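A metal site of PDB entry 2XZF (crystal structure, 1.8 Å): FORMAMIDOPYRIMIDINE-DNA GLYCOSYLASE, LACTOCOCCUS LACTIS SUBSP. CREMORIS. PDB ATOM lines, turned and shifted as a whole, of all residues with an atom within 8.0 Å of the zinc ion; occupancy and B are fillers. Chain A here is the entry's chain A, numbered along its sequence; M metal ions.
Of the 18 residues printed, 4 come within 4 Å of the zinc ion.
The zinc ion is bound by SG of Cys 265 (2.2 Å), SG of Cys 245 (2.3 Å), SG of Cys 248 (2.3 Å) and SG of Cys 268 (2.4 Å).
The zinc ion has four donor atoms within binding distance.
The side-chain sulfur (SG) of Cys 265 sits close to the backbone NH (N) of Val 267, 3.5 Å away.
The backbone NH of Cys 265 sits at hydrogen-bond distance from the side-chain amide oxygen of Gln 269 (2.8 Å).
The backbone NH of Arg 247 sits close to the side-chain sulfur of Cys 245 (3.4 Å).
The indole nitrogen (NE1) of Trp 179 sits close to the side-chain sulfur (SG) of Cys 245, 3.4 Å away.
The backbone NH (N) of Cys 245 lies within hydrogen-bond range of the backbone carbonyl oxygen (O) of Ala 250.
SG of Cys 248 lies close to N of Ala 250.
The guanidinium group (NE) of Arg 247 lies close to the side-chain sulfur (SG) of Cys 268 (3.4 Å).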
ATOM      1  N   TRP A 179       2.532  -1.004  -6.314  1.00  0.00           N
ATOM      2  CA  TRP A 179       3.090  -2.075  -7.143  1.00  0.00           C
ATOM      3  C   TRP A 179       3.956  -2.971  -6.270  1.00  0.00           C
ATOM      4  O   TRP A 179       3.850  -4.198  -6.325  1.00  0.00           O
ATOM      5  CB  TRP A 179       3.907  -1.504  -8.307  1.00  0.00           C
ATOM      6  CG  TRP A 179       4.589  -2.575  -9.147  1.00  0.00           C
ATOM      7  CD1 TRP A 179       4.071  -3.209 -10.241  1.00  0.00           C
ATOM      8  CD2 TRP A 179       5.907  -3.105  -8.951  1.00  0.00           C
ATOM      9  NE1 TRP A 179       4.988  -4.116 -10.736  1.00  0.00           N
ATOM     10  CE2 TRP A 179       6.129  -4.052  -9.974  1.00  0.00           C
ATOM     11  CE3 TRP A 179       6.925  -2.862  -8.034  1.00  0.00           C
ATOM     12  CZ2 TRP A 179       7.323  -4.774 -10.096  1.00  0.00           C
ATOM     13  CZ3 TRP A 179       8.113  -3.581  -8.143  1.00  0.00           C
ATOM     14  CH2 TRP A 179       8.305  -4.523  -9.171  1.00  0.00           C
ATOM     15  N   LYS A 182       1.927  -5.157  -4.160  1.00  0.00           N
ATOM     16  CA  LYS A 182       0.975  -5.988  -4.921  1.00  0.00           C
ATOM     17  C   LYS A 182      -0.483  -5.685  -4.587  1.00  0.00           C
ATOM     18  O   LYS A 182      -1.299  -6.594  -4.406  1.00  0.00           O
ATOM     19  CB  LYS A 182       1.311  -7.479  -4.735  1.00  0.00           C
ATOM     20  CG  LYS A 182       2.725  -7.828  -5.218  1.00  0.00           C
ATOM     21  CD  LYS A 182       3.078  -9.300  -4.974  1.00  0.00           C
ATOM     22  CE  LYS A 182       4.520  -9.575  -5.382  1.00  0.00           C
ATOM     23  NZ  LYS A 182       4.931 -11.011  -5.184  1.00  0.00           N
ATOM     24  N   VAL A 237       6.812   1.420 -12.219  1.00  0.00           N
ATOM     25  CA  VAL A 237       5.522   1.616 -12.891  1.00  0.00           C
ATOM     26  C   VAL A 237       5.219   3.053 -13.309  1.00  0.00           C
ATOM     27  O   VAL A 237       4.630   3.282 -14.374  1.00  0.00           O
ATOM     28  CB  VAL A 237       4.322   1.090 -12.057  1.00  0.00           C
ATOM     29  CG1 VAL A 237       4.340  -0.440 -11.986  1.00  0.00           C
ATOM     30  CG2 VAL A 237       4.299   1.708 -10.624  1.00  0.00           C
ATOM     31  N   LYS A 244       7.041  -3.492 -19.855  1.00  0.00           N
ATOM     32  CA  LYS A 244       6.717  -4.756 -19.178  1.00  0.00           C
ATOM     33  C   LYS A 244       7.034  -4.689 -17.692  1.00  0.00           C
ATOM     34  O   LYS A 244       8.022  -4.078 -17.270  1.00  0.00           O
ATOM     35  CB  LYS A 244       7.456  -5.931 -19.834  1.00  0.00           C
ATOM     36  CG  LYS A 244       7.346  -5.992 -21.352  1.00  0.00           C
ATOM     37  CD  LYS A 244       5.899  -5.953 -21.857  1.00  0.00           C
ATOM     38  CE  LYS A 244       5.856  -6.161 -23.396  1.00  0.00           C
ATOM     39  NZ  LYS A 244       4.478  -6.254 -23.986  1.00  0.00           N
ATOM     40  N   CYS A 245       6.163  -5.283 -16.880  1.00  0.00           N
ATOM     41  CA  CYS A 245       6.395  -5.404 -15.455  1.00  0.00           C
ATOM     42  C   CYS A 245       7.689  -6.179 -15.214  1.00  0.00           C
ATOM     43  O   CYS A 245       7.905  -7.219 -15.810  1.00  0.00           O
ATOM     44  CB  CYS A 245       5.223  -6.165 -14.820  1.00  0.00           C
ATOM     45  SG  CYS A 245       5.437  -6.488 -13.076  1.00  0.00           S
ATOM     46  N   SER A 246       8.555  -5.680 -14.338  1.00  0.00           N
ATOM     47  CA  SER A 246       9.809  -6.392 -14.064  1.00  0.00           C
ATOM     48  C   SER A 246       9.613  -7.760 -13.383  1.00  0.00           C
ATOM     49  O   SER A 246      10.481  -8.619 -13.465  1.00  0.00           O
ATOM     50  CB  SER A 246      10.741  -5.528 -13.209  1.00  0.00           C
ATOM     51  OG  SER A 246      10.203  -5.377 -11.906  1.00  0.00           O
ATOM     52  N   ARG A 247       8.470  -7.960 -12.728  1.00  0.00           N
ATOM     53  CA  ARG A 247       8.210  -9.217 -12.025  1.00  0.00           C
ATOM     54  C   ARG A 247       7.582 -10.288 -12.909  1.00  0.00           C
ATOM     55  O   ARG A 247       8.074 -11.416 -12.947  1.00  0.00           O
ATOM     56  CB  ARG A 247       7.330  -8.992 -10.777  1.00  0.00           C
ATOM     57  CG  ARG A 247       8.116  -8.560  -9.541  1.00  0.00           C
ATOM     58  CD  ARG A 247       7.224  -8.437  -8.293  1.00  0.00           C
ATOM     59  NE  ARG A 247       6.011  -7.680  -8.599  1.00  0.00           N
ATOM     60  CZ  ARG A 247       5.457  -6.779  -7.790  1.00  0.00           C
ATOM     61  NH1 ARG A 247       5.988  -6.515  -6.603  1.00  0.00           N
ATOM     62  NH2 ARG A 247       4.367  -6.159  -8.181  1.00  0.00           N
ATOM     63  N   CYS A 248       6.510  -9.951 -13.627  1.00  0.00           N
ATOM     64  CA  CYS A 248       5.760 -10.979 -14.352  1.00  0.00           C
ATOM     65  C   CYS A 248       5.752 -10.797 -15.867  1.00  0.00           C
ATOM     66  O   CYS A 248       5.336 -11.708 -16.593  1.00  0.00           O
ATOM     67  CB  CYS A 248       4.321 -11.005 -13.869  1.00  0.00           C
ATOM     68  SG  CYS A 248       3.402  -9.557 -14.396  1.00  0.00           S
ATOM     69  N   GLY A 249       6.184  -9.642 -16.347  1.00  0.00           N
ATOM     70  CA  GLY A 249       6.289  -9.426 -17.775  1.00  0.00           C
ATOM     71  C   GLY A 249       5.040  -8.871 -18.430  1.00  0.00           C
ATOM     72  O   GLY A 249       5.041  -8.639 -19.624  1.00  0.00           O
ATOM     73  N   ALA A 250       3.986  -8.640 -17.651  1.00  0.00           N
ATOM     74  CA  ALA A 250       2.745  -8.074 -18.218  1.00  0.00           C
ATOM     75  C   ALA A 250       2.949  -6.596 -18.536  1.00  0.00           C
ATOM     76  O   ALA A 250       3.766  -5.942 -17.882  1.00  0.00           O
ATOM     77  CB  ALA A 250       1.582  -8.259 -17.240  1.00  0.00           C
ATOM     78  N   GLU A 251       2.247  -6.054 -19.537  1.00  0.00           N
ATOM     79  CA  GLU A 251       2.330  -4.607 -19.814  1.00  0.00           C
ATOM     80  C   GLU A 251       1.741  -3.756 -18.683  1.00  0.00           C
ATOM     81  O   GLU A 251       0.626  -3.982 -18.229  1.00  0.00           O
ATOM     82  CB  GLU A 251       1.636  -4.201 -21.127  1.00  0.00           C
ATOM     83  CG  GLU A 251       2.315  -4.696 -22.367  1.00  0.00           C
ATOM     84  CD  GLU A 251       2.030  -3.838 -23.607  1.00  0.00           C
ATOM     85  OE1 GLU A 251       1.236  -2.874 -23.554  1.00  0.00           O
ATOM     86  OE2 GLU A 251       2.656  -4.117 -24.631  1.00  0.00           O
ATOM     87  N   ILE A 252       2.506  -2.755 -18.265  1.00  0.00           N
ATOM     88  CA  ILE A 252       2.005  -1.778 -17.308  1.00  0.00           C
ATOM     89  C   ILE A 252       0.879  -0.961 -17.963  1.00  0.00           C
ATOM     90  O   ILE A 252       1.000  -0.506 -19.112  1.00  0.00           O
ATOM     91  CB  ILE A 252       3.128  -0.827 -16.827  1.00  0.00           C
ATOM     92  CG1 ILE A 252       4.241  -1.617 -16.144  1.00  0.00           C
ATOM     93  CG2 ILE A 252       2.570   0.274 -15.925  1.00  0.00           C
ATOM     94  CD1 ILE A 252       3.760  -2.594 -15.066  1.00  0.00           C
ATOM     95  N   PHE A 264      -0.089   0.756 -13.075  1.00  0.00           N
ATOM     96  CA  PHE A 264      -0.079  -0.492 -12.294  1.00  0.00           C
ATOM     97  C   PHE A 264       0.118  -1.712 -13.204  1.00  0.00           C
ATOM     98  O   PHE A 264      -0.058  -1.635 -14.427  1.00  0.00           O
ATOM     99  CB  PHE A 264      -1.399  -0.638 -11.529  1.00  0.00           C
ATOM    100  CG  PHE A 264      -2.568  -0.975 -12.420  1.00  0.00           C
ATOM    101  CD1 PHE A 264      -3.104  -0.001 -13.273  1.00  0.00           C
ATOM    102  CD2 PHE A 264      -3.118  -2.248 -12.432  1.00  0.00           C
ATOM    103  CE1 PHE A 264      -4.153  -0.297 -14.123  1.00  0.00           C
ATOM    104  CE2 PHE A 264      -4.179  -2.551 -13.278  1.00  0.00           C
ATOM    105  CZ  PHE A 264      -4.696  -1.575 -14.123  1.00  0.00           C
ATOM    106  N   CYS A 265       0.482  -2.833 -12.589  1.00  0.00           N
ATOM    107  CA  CYS A 265       0.537  -4.106 -13.315  1.00  0.00           C
ATOM    108  C   CYS A 265      -0.743  -4.867 -12.981  1.00  0.00           C
ATOM    109  O   CYS A 265      -1.002  -5.125 -11.810  1.00  0.00           O
ATOM    110  CB  CYS A 265       1.733  -4.948 -12.860  1.00  0.00           C
ATOM    111  SG  CYS A 265       1.730  -6.661 -13.540  1.00  0.00           S
ATOM    112  N   PRO A 266      -1.545  -5.213 -14.007  1.00  0.00           N
ATOM    113  CA  PRO A 266      -2.832  -5.902 -13.815  1.00  0.00           C
ATOM    114  C   PRO A 266      -2.696  -7.331 -13.303  1.00  0.00           C
ATOM    115  O   PRO A 266      -3.690  -7.899 -12.843  1.00  0.00           O
ATOM    116  CB  PRO A 266      -3.458  -5.909 -15.215  1.00  0.00           C
ATOM    117  CG  PRO A 266      -2.671  -4.916 -16.006  1.00  0.00           C
ATOM    118  CD  PRO A 266      -1.308  -4.889 -15.417  1.00  0.00           C
ATOM    119  N   VAL A 267      -1.509  -7.928 -13.413  1.00  0.00           N
ATOM    120  CA  VAL A 267      -1.285  -9.288 -12.925  1.00  0.00           C
ATOM    121  C   VAL A 267      -0.894  -9.231 -11.461  1.00  0.00           C
ATOM    122  O   VAL A 267      -1.489  -9.911 -10.612  1.00  0.00           O
ATOM    123  CB  VAL A 267      -0.171 -10.000 -13.727  1.00  0.00           C
ATOM    124  CG1 VAL A 267       0.204 -11.330 -13.081  1.00  0.00           C
ATOM    125  CG2 VAL A 267      -0.649 -10.235 -15.169  1.00  0.00           C
ATOM    126  N   CYS A 268       0.121  -8.427 -11.159  1.00  0.00           N
ATOM    127  CA  CYS A 268       0.672  -8.345  -9.805  1.00  0.00           C
ATOM    128  C   CYS A 268      -0.276  -7.620  -8.852  1.00  0.00           C
ATOM    129  O   CYS A 268      -0.216  -7.849  -7.649  1.00  0.00           O
ATOM    130  CB  CYS A 268       2.011  -7.603  -9.815  1.00  0.00           C
ATOM    131  SG  CYS A 268       3.377  -8.534 -10.594  1.00  0.00           S
ATOM    132  N   GLN A 269      -1.098  -6.728  -9.395  1.00  0.00           N
ATOM    133  CA  GLN A 269      -2.028  -5.945  -8.586  1.00  0.00           C
ATOM    134  C   GLN A 269      -3.460  -6.279  -8.973  1.00  0.00           C
ATOM    135  O   GLN A 269      -4.088  -5.584  -9.763  1.00  0.00           O
ATOM    136  CB  GLN A 269      -1.738  -4.441  -8.718  1.00  0.00           C
ATOM    137  CG  GLN A 269      -0.309  -4.084  -8.329  1.00  0.00           C
ATOM    138  CD  GLN A 269       0.094  -2.709  -8.825  1.00  0.00           C
ATOM    139  OE1 GLN A 269       0.790  -2.566  -9.840  1.00  0.00           O
ATOM    140  NE2 GLN A 269      -0.341  -1.672  -8.109  1.00  0.00           N
HETATM  141 ZN    ZN M   1       3.517  -7.811 -12.829  1.00  0.00          ZN
